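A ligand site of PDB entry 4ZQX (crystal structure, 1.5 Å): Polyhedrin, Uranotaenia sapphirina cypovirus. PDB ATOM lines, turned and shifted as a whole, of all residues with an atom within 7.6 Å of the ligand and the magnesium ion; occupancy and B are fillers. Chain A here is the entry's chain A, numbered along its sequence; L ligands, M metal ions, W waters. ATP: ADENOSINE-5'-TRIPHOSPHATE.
An oxygen (O3G) of the ligand sits at hydrogen-bond distance from the backbone NH (N) of Arg 158 (2.9 Å). OG of Ser 154 sits at hydrogen-bond distance from O2G of the ligand, 2.7 Å away. O of Ser 234 sits at hydrogen-bond distance from N6 of the ligand (3.0 Å). An oxygen (O2G) of the ligand is in hydrogen-bond range of the backbone NH (N) of Ser 154 (2.9 Å). O3B of the ligand sits at hydrogen-bond distance from N of Cys 155 (3.2 Å). The backbone NH (N) of Gly 157 lies within hydrogen-bond range of an oxygen (O3G) of the ligand. A nitrogen (N1) of the ligand is in hydrogen-bond range of the side-chain hydroxyl (OG) of Ser 234, 3.4 Å away. An oxygen (O3G) of the ligand sits at hydrogen-bond distance from the backbone NH of Gly 156 (3.0 Å).
The side-chain sulfur (SG) of Cys 159 lies within hydrogen-bond range of the guanidinium group (NH1) of Arg 107, 3.7 Å away. O of Glu 160 lies within hydrogen-bond range of N of Leu 152 (3.2 Å). The side-chain hydroxyl (OG) of Ser 154 is in hydrogen-bond range of the backbone NH (N) of Gly 157 (3.2 Å). The side-chain hydroxyl (OG) of Ser 154 sits at hydrogen-bond distance from the backbone NH (N) of Arg 158 (2.8 Å). The backbone carbonyl oxygen (O) of Pro 153 lies within hydrogen-bond range of the side-chain hydroxyl (OG1) of Thr 228 (2.8 Å). The guanidinium group (NH1) of Arg 158 sits at hydrogen-bond distance from the backbone carbonyl oxygen (O) of Gly 156, 3.2 Å away. OD1 of Asn 17 lies close to O of Cys 155 (3.4 Å). O of Ser 154 lies within hydrogen-bond range of NH2 of Arg 107, at 3.0 Å.
N of Pro 153 sits close to O4' of the ligand, 3.5 Å away. Merely in contact with the ligand: Asp 151 (3.5 Å), Leu 152 (3.5 Å), Cys 159 (3.997 Å), Leu 230 (3.6 Å) and Ile 236 (3.8 Å). Hydrophobic or aromatic side chains that line the ligand: Pro 153, Leu 230 and Ile 236. 12 residues have an atom within 4 Å of the ligand: Asp 151, Leu 152, Pro 153, Ser 154, Cys 155, Gly 156, Gly 157, Arg 158, Cys 159, Leu 230, Ser 234 and Ile 236.
No residue comes within 4 Å of the magnesium ion. The nearest printed residue that does not touch the magnesium ion is Arg 158 (5.3 Å).
O1G of the ligand binds the magnesium ion (2.0 Å). The magnesium ion is bound by O2A of the ligand, 2.0 Å away. An oxygen (O2B) of the ligand is bound to the magnesium ion, 2.1 Å away. The magnesium ion is bound by water W4 (2.2 Å). Water W2 is bound to the magnesium ion, 2.4 Å away.
Water W1 lies within hydrogen-bond range of O of Leu 152 (2.7 Å), O2G of the ligand (2.7 Å), N of Glu 160 (2.9 Å) and N of Cys 159 (3.3 Å). Water W5 lies within hydrogen-bond range of O of Asp 151 (2.8 Å) and N3 of the ligand (2.9 Å). Water W3 lies within hydrogen-bond range of N6 of the ligand (3.1 Å) and N of Ile 236 (3.1 Å).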
ATOM      1  N   ASN A  17      15.489 -27.242  23.282  1.00  0.00           N
ATOM      2  CA  ASN A  17      15.847 -26.544  22.053  1.00  0.00           C
ATOM      3  C   ASN A  17      16.499 -27.451  21.018  1.00  0.00           C
ATOM      4  O   ASN A  17      16.220 -27.314  19.834  1.00  0.00           O
ATOM      5  CB  ASN A  17      16.803 -25.387  22.357  1.00  0.00           C
ATOM      6  CG  ASN A  17      16.120 -24.261  23.097  1.00  0.00           C
ATOM      7  OD1 ASN A  17      14.885 -24.160  23.104  1.00  0.00           O
ATOM      8  ND2 ASN A  17      16.907 -23.393  23.714  1.00  0.00           N
ATOM      9  N   ARG A 107       8.957 -26.921  11.138  1.00  0.00           N
ATOM     10  CA  ARG A 107       9.791 -26.777  12.322  1.00  0.00           C
ATOM     11  C   ARG A 107      10.632 -28.020  12.508  1.00  0.00           C
ATOM     12  O   ARG A 107      10.107 -29.122  12.581  1.00  0.00           O
ATOM     13  CB  ARG A 107       8.938 -26.535  13.583  1.00  0.00           C
ATOM     14  CG  ARG A 107       9.741 -26.053  14.789  1.00  0.00           C
ATOM     15  CD  ARG A 107       8.962 -26.186  16.116  1.00  0.00           C
ATOM     16  NE  ARG A 107       9.611 -25.443  17.195  1.00  0.00           N
ATOM     17  CZ  ARG A 107      10.600 -25.919  17.954  1.00  0.00           C
ATOM     18  NH1 ARG A 107      11.046 -27.154  17.778  1.00  0.00           N
ATOM     19  NH2 ARG A 107      11.140 -25.152  18.897  1.00  0.00           N
ATOM     20  N   VAL A 150      10.114 -17.727   5.040  1.00  0.00           N
ATOM     21  CA  VAL A 150      10.131 -16.596   5.949  1.00  0.00           C
ATOM     22  C   VAL A 150      10.523 -17.129   7.345  1.00  0.00           C
ATOM     23  O   VAL A 150       9.912 -18.066   7.825  1.00  0.00           O
ATOM     24  CB  VAL A 150       8.729 -15.956   6.023  1.00  0.00           C
ATOM     25  CG1 VAL A 150       8.677 -14.831   7.054  1.00  0.00           C
ATOM     26  CG2 VAL A 150       8.307 -15.433   4.636  1.00  0.00           C
ATOM     27  N   ASP A 151      11.527 -16.533   7.979  1.00  0.00           N
ATOM     28  CA  ASP A 151      11.982 -17.016   9.297  1.00  0.00           C
ATOM     29  C   ASP A 151      11.040 -16.532  10.375  1.00  0.00           C
ATOM     30  O   ASP A 151      10.599 -15.380  10.324  1.00  0.00           O
ATOM     31  CB  ASP A 151      13.399 -16.512   9.639  1.00  0.00           C
ATOM     32  CG  ASP A 151      14.453 -16.989   8.666  1.00  0.00           C
ATOM     33  OD1 ASP A 151      14.197 -17.935   7.890  1.00  0.00           O
ATOM     34  OD2 ASP A 151      15.557 -16.411   8.679  1.00  0.00           O
ATOM     35  N   LEU A 152      10.737 -17.412  11.350  1.00  0.00           N
ATOM     36  CA  LEU A 152       9.877 -17.081  12.489  1.00  0.00           C
ATOM     37  C   LEU A 152      10.502 -17.611  13.770  1.00  0.00           C
ATOM     38  O   LEU A 152      11.263 -18.564  13.731  1.00  0.00           O
ATOM     39  CB  LEU A 152       8.492 -17.689  12.326  1.00  0.00           C
ATOM     40  CG  LEU A 152       7.591 -17.115  11.226  1.00  0.00           C
ATOM     41  CD1 LEU A 152       6.262 -17.844  11.196  1.00  0.00           C
ATOM     42  CD2 LEU A 152       7.366 -15.608  11.402  1.00  0.00           C
ATOM     43  N   PRO A 153      10.168 -16.977  14.918  1.00  0.00           N
ATOM     44  CA  PRO A 153      10.749 -17.432  16.192  1.00  0.00           C
ATOM     45  C   PRO A 153      10.356 -18.853  16.544  1.00  0.00           C
ATOM     46  O   PRO A 153       9.178 -19.192  16.406  1.00  0.00           O
ATOM     47  CB  PRO A 153      10.143 -16.472  17.212  1.00  0.00           C
ATOM     48  CG  PRO A 153       9.797 -15.267  16.450  1.00  0.00           C
ATOM     49  CD  PRO A 153       9.411 -15.739  15.078  1.00  0.00           C
ATOM     50  N   SER A 154      11.325 -19.657  16.995  1.00  0.00           N
ATOM     51  CA  SER A 154      11.049 -20.989  17.508  1.00  0.00           C
ATOM     52  C   SER A 154      11.445 -21.102  18.979  1.00  0.00           C
ATOM     53  O   SER A 154      11.544 -22.201  19.530  1.00  0.00           O
ATOM     54  CB  SER A 154      11.780 -22.042  16.673  1.00  0.00           C
ATOM     55  OG  SER A 154      13.182 -21.958  16.816  1.00  0.00           O
ATOM     56  N   CYS A 155      11.663 -19.952  19.606  1.00  0.00           N
ATOM     57  CA  CYS A 155      11.874 -19.891  21.053  1.00  0.00           C
ATOM     58  C   CYS A 155      13.093 -20.685  21.540  1.00  0.00           C
ATOM     59  O   CYS A 155      13.072 -21.314  22.608  1.00  0.00           O
ATOM     60  CB  CYS A 155      10.599 -20.332  21.778  1.00  0.00           C
ATOM     61  SG  CYS A 155       9.207 -19.233  21.471  1.00  0.00           S
ATOM     62  N   GLY A 156      14.161 -20.608  20.751  1.00  0.00           N
ATOM     63  CA  GLY A 156      15.452 -21.174  21.133  1.00  0.00           C
ATOM     64  C   GLY A 156      15.908 -22.272  20.195  1.00  0.00           C
ATOM     65  O   GLY A 156      17.072 -22.678  20.236  1.00  0.00           O
ATOM     66  N   GLY A 157      15.003 -22.759  19.364  1.00  0.00           N
ATOM     67  CA  GLY A 157      15.320 -23.870  18.476  1.00  0.00           C
ATOM     68  C   GLY A 157      16.064 -23.470  17.208  1.00  0.00           C
ATOM     69  O   GLY A 157      16.706 -24.306  16.591  1.00  0.00           O
ATOM     70  N   ARG A 158      15.988 -22.194  16.850  1.00  0.00           N
ATOM     71  CA  ARG A 158      16.552 -21.720  15.585  1.00  0.00           C
ATOM     72  C   ARG A 158      16.097 -22.583  14.406  1.00  0.00           C
ATOM     73  O   ARG A 158      16.892 -22.895  13.516  1.00  0.00           O
ATOM     74  CB  ARG A 158      18.098 -21.724  15.647  1.00  0.00           C
ATOM     75  CG  ARG A 158      18.659 -21.090  16.912  1.00  0.00           C
ATOM     76  CD  ARG A 158      20.189 -21.177  16.989  1.00  0.00           C
ATOM     77  NE  ARG A 158      20.714 -22.541  16.919  1.00  0.00           N
ATOM     78  CZ  ARG A 158      20.634 -23.446  17.892  1.00  0.00           C
ATOM     79  NH1 ARG A 158      20.016 -23.161  19.029  1.00  0.00           N
ATOM     80  NH2 ARG A 158      21.165 -24.651  17.711  1.00  0.00           N
ATOM     81  N   CYS A 159      14.831 -22.985  14.392  1.00  0.00           N
ATOM     82  CA  CYS A 159      14.406 -23.992  13.432  1.00  0.00           C
ATOM     83  C   CYS A 159      12.978 -23.929  12.920  1.00  0.00           C
ATOM     84  O   CYS A 159      12.436 -24.954  12.534  1.00  0.00           O
ATOM     85  CB  CYS A 159      14.665 -25.375  14.046  1.00  0.00           C
ATOM     86  SG  CYS A 159      13.622 -25.829  15.463  1.00  0.00           S
ATOM     87  N   GLU A 160      12.378 -22.741  12.876  1.00  0.00           N
ATOM     88  CA  GLU A 160      11.045 -22.621  12.247  1.00  0.00           C
ATOM     89  C   GLU A 160      11.077 -21.608  11.098  1.00  0.00           C
ATOM     90  O   GLU A 160      11.634 -20.504  11.232  1.00  0.00           O
ATOM     91  CB  GLU A 160       9.957 -22.233  13.248  1.00  0.00           C
ATOM     92  CG  GLU A 160       8.568 -22.213  12.573  1.00  0.00           C
ATOM     93  CD  GLU A 160       7.436 -21.722  13.464  1.00  0.00           C
ATOM     94  OE1 GLU A 160       7.512 -21.902  14.684  1.00  0.00           O
ATOM     95  OE2 GLU A 160       6.480 -21.147  12.920  1.00  0.00           O
ATOM     96  N   THR A 228       4.952 -21.330  16.331  1.00  0.00           N
ATOM     97  CA  THR A 228       4.672 -19.904  16.247  1.00  0.00           C
ATOM     98  C   THR A 228       3.965 -19.614  14.928  1.00  0.00           C
ATOM     99  O   THR A 228       4.362 -20.132  13.903  1.00  0.00           O
ATOM    100  CB  THR A 228       5.993 -19.105  16.338  1.00  0.00           C
ATOM    101  OG1 THR A 228       6.672 -19.479  17.549  1.00  0.00           O
ATOM    102  CG2 THR A 228       5.720 -17.624  16.352  1.00  0.00           C
ATOM    103  N   MET A 229       2.891 -18.836  14.961  1.00  0.00           N
ATOM    104  CA  MET A 229       2.184 -18.467  13.743  1.00  0.00           C
ATOM    105  C   MET A 229       2.136 -16.962  13.602  1.00  0.00           C
ATOM    106  O   MET A 229       2.246 -16.237  14.588  1.00  0.00           O
ATOM    107  CB  MET A 229       0.773 -19.070  13.756  1.00  0.00           C
ATOM    108  CG  MET A 229       0.812 -20.566  13.733  1.00  0.00           C
ATOM    109  SD  MET A 229      -0.812 -21.299  13.580  1.00  0.00           S
ATOM    110  CE  MET A 229      -0.346 -23.007  13.527  1.00  0.00           C
ATOM    111  N   LEU A 230       1.954 -16.504  12.367  1.00  0.00           N
ATOM    112  CA  LEU A 230       1.956 -15.098  12.036  1.00  0.00           C
ATOM    113  C   LEU A 230       0.581 -14.727  11.510  1.00  0.00           C
ATOM    114  O   LEU A 230       0.042 -15.424  10.648  1.00  0.00           O
ATOM    115  CB  LEU A 230       2.999 -14.825  10.950  1.00  0.00           C
ATOM    116  CG  LEU A 230       3.374 -13.382  10.701  1.00  0.00           C
ATOM    117  CD1 LEU A 230       4.133 -12.844  11.889  1.00  0.00           C
ATOM    118  CD2 LEU A 230       4.209 -13.235   9.431  1.00  0.00           C
ATOM    119  N   ASP A 231       0.019 -13.625  12.019  1.00  0.00           N
ATOM    120  CA  ASP A 231      -1.310 -13.200  11.581  1.00  0.00           C
ATOM    121  C   ASP A 231      -1.214 -12.137  10.487  1.00  0.00           C
ATOM    122  O   ASP A 231      -0.120 -11.793  10.026  1.00  0.00           O
ATOM    123  CB  ASP A 231      -2.179 -12.724  12.778  1.00  0.00           C
ATOM    124  CG  ASP A 231      -1.699 -11.437  13.410  1.00  0.00           C
ATOM    125  OD1 ASP A 231      -0.947 -10.669  12.764  1.00  0.00           O
ATOM    126  OD2 ASP A 231      -2.085 -11.189  14.575  1.00  0.00           O
ATOM    127  N   PHE A 233      -1.585  -9.079  10.593  1.00  0.00           N
ATOM    128  CA  PHE A 233      -1.013  -7.823  11.077  1.00  0.00           C
ATOM    129  C   PHE A 233       0.488  -7.965  11.329  1.00  0.00           C
ATOM    130  O   PHE A 233       1.110  -7.076  11.906  1.00  0.00           O
ATOM    131  CB  PHE A 233      -1.748  -7.376  12.353  1.00  0.00           C
ATOM    132  CG  PHE A 233      -3.240  -7.390  12.216  1.00  0.00           C
ATOM    133  CD1 PHE A 233      -3.887  -6.482  11.383  1.00  0.00           C
ATOM    134  CD2 PHE A 233      -3.995  -8.325  12.893  1.00  0.00           C
ATOM    135  CE1 PHE A 233      -5.266  -6.497  11.242  1.00  0.00           C
ATOM    136  CE2 PHE A 233      -5.368  -8.363  12.748  1.00  0.00           C
ATOM    137  CZ  PHE A 233      -6.012  -7.442  11.919  1.00  0.00           C
ATOM    138  N   SER A 234       1.045  -9.081  10.877  1.00  0.00           N
ATOM    139  CA  SER A 234       2.440  -9.455  11.117  1.00  0.00           C
ATOM    140  C   SER A 234       2.779  -9.583  12.590  1.00  0.00           C
ATOM    141  O   SER A 234       3.909  -9.305  12.976  1.00  0.00           O
ATOM    142  CB  SER A 234       3.391  -8.445  10.458  1.00  0.00           C
ATOM    143  OG  SER A 234       4.676  -9.039  10.313  1.00  0.00           O
ATOM    144  N   VAL A 235       1.814 -10.008  13.402  1.00  0.00           N
ATOM    145  CA  VAL A 235       2.057 -10.235  14.839  1.00  0.00           C
ATOM    146  C   VAL A 235       2.146 -11.749  15.083  1.00  0.00           C
ATOM    147  O   VAL A 235       1.355 -12.515  14.512  1.00  0.00           O
ATOM    148  CB  VAL A 235       0.934  -9.610  15.705  1.00  0.00           C
ATOM    149  CG1 VAL A 235       1.073 -10.000  17.180  1.00  0.00           C
ATOM    150  CG2 VAL A 235       0.957  -8.077  15.556  1.00  0.00           C
ATOM    151  N   ILE A 236       3.089 -12.171  15.916  1.00  0.00           N
ATOM    152  CA  ILE A 236       3.281 -13.601  16.185  1.00  0.00           C
ATOM    153  C   ILE A 236       2.421 -14.098  17.345  1.00  0.00           C
ATOM    154  O   ILE A 236       2.094 -13.335  18.262  1.00  0.00           O
ATOM    155  CB  ILE A 236       4.752 -13.962  16.463  1.00  0.00           C
ATOM    156  CG1 ILE A 236       5.290 -13.233  17.712  1.00  0.00           C
ATOM    157  CG2 ILE A 236       5.571 -13.675  15.225  1.00  0.00           C
ATOM    158  CD1 ILE A 236       6.739 -13.604  18.050  1.00  0.00           C
ATOM    159  N   HIS A 237       2.076 -15.382  17.283  1.00  0.00           N
ATOM    160  CA  HIS A 237       1.280 -16.043  18.310  1.00  0.00           C
ATOM    161  C   HIS A 237       1.861 -17.401  18.605  1.00  0.00           C
ATOM    162  O   HIS A 237       2.421 -18.017  17.712  1.00  0.00           O
ATOM    163  CB  HIS A 237      -0.157 -16.181  17.846  1.00  0.00           C
ATOM    164  CG  HIS A 237      -0.781 -14.883  17.455  1.00  0.00           C
ATOM    165  ND1 HIS A 237      -1.461 -14.090  18.351  1.00  0.00           N
ATOM    166  CD2 HIS A 237      -0.745 -14.194  16.289  1.00  0.00           C
ATOM    167  CE1 HIS A 237      -1.872 -12.991  17.740  1.00  0.00           C
ATOM    168  NE2 HIS A 237      -1.432 -13.026  16.492  1.00  0.00           N
ATOM    169  OXT HIS A 237       1.781 -17.871  19.741  1.00  0.00           O
HETATM  170  PG  ATP L   1      14.882 -18.792  17.304  1.00  0.00           P
HETATM  171  O1G ATP L   1      15.784 -17.701  16.796  1.00  0.00           O
HETATM  172  O2G ATP L   1      14.076 -19.526  16.246  1.00  0.00           O
HETATM  173  O3G ATP L   1      15.545 -19.732  18.297  1.00  0.00           O
HETATM  174  PB  ATP L   1      13.787 -16.691  18.949  1.00  0.00           P
HETATM  175  O1B ATP L   1      12.660 -16.772  19.952  1.00  0.00           O
HETATM  176  O2B ATP L   1      15.209 -16.479  19.407  1.00  0.00           O
HETATM  177  O3B ATP L   1      13.674 -18.035  18.057  1.00  0.00           O
HETATM  178  PA  ATP L   1      14.189 -14.347  17.242  1.00  0.00           P
HETATM  179  O1A ATP L   1      13.827 -13.096  17.998  1.00  0.00           O
HETATM  180  O2A ATP L   1      15.646 -14.734  17.077  1.00  0.00           O
HETATM  181  O3A ATP L   1      13.330 -15.570  17.860  1.00  0.00           O
HETATM  182  O5' ATP L   1      13.551 -14.197  15.753  1.00  0.00           O
HETATM  183  C5' ATP L   1      13.706 -15.227  14.765  1.00  0.00           C
HETATM  184  C4' ATP L   1      13.274 -14.654  13.429  1.00  0.00           C
HETATM  185  O4' ATP L   1      11.877 -14.356  13.445  1.00  0.00           O
HETATM  186  C3' ATP L   1      13.983 -13.345  13.103  1.00  0.00           C
HETATM  187  O3' ATP L   1      14.448 -13.397  11.749  1.00  0.00           O
HETATM  188  C2' ATP L   1      12.924 -12.272  13.237  1.00  0.00           C
HETATM  189  O2' ATP L   1      13.087 -11.145  12.366  1.00  0.00           O
HETATM  190  C1' ATP L   1      11.653 -13.046  12.921  1.00  0.00           C
HETATM  191  N9  ATP L   1      10.494 -12.360  13.544  1.00  0.00           N
HETATM  192  C8  ATP L   1      10.312 -12.105  14.860  1.00  0.00           C
HETATM  193  N7  ATP L   1       9.145 -11.449  15.076  1.00  0.00           N
HETATM  194  C5  ATP L   1       8.560 -11.285  13.868  1.00  0.00           C
HETATM  195  C6  ATP L   1       7.327 -10.677  13.382  1.00  0.00           C
HETATM  196  N6  ATP L   1       6.504 -10.121  14.297  1.00  0.00           N
HETATM  197  N1  ATP L   1       7.069 -10.695  12.048  1.00  0.00           N
HETATM  198  C2  ATP L   1       7.927 -11.266  11.180  1.00  0.00           C
HETATM  199  N3  ATP L   1       9.084 -11.840  11.565  1.00  0.00           N
HETATM  200  C4  ATP L   1       9.454 -11.883  12.863  1.00  0.00           C
HETATM  201 MG    MG M   1      16.675 -16.291  17.906  1.00  0.00          MG
HETATM  202  O   HOH W   1      13.429 -20.144  13.652  1.00  0.00           O
HETATM  203  O   HOH W   2      17.396 -14.744  19.560  1.00  0.00           O
HETATM  204  O   HOH W   3       4.903  -9.830  16.913  1.00  0.00           O
HETATM  205  O   HOH W   4      17.509 -18.005  19.099  1.00  0.00           O
HETATM  206  O   HOH W   5      10.604 -12.820   9.302  1.00  0.00           O
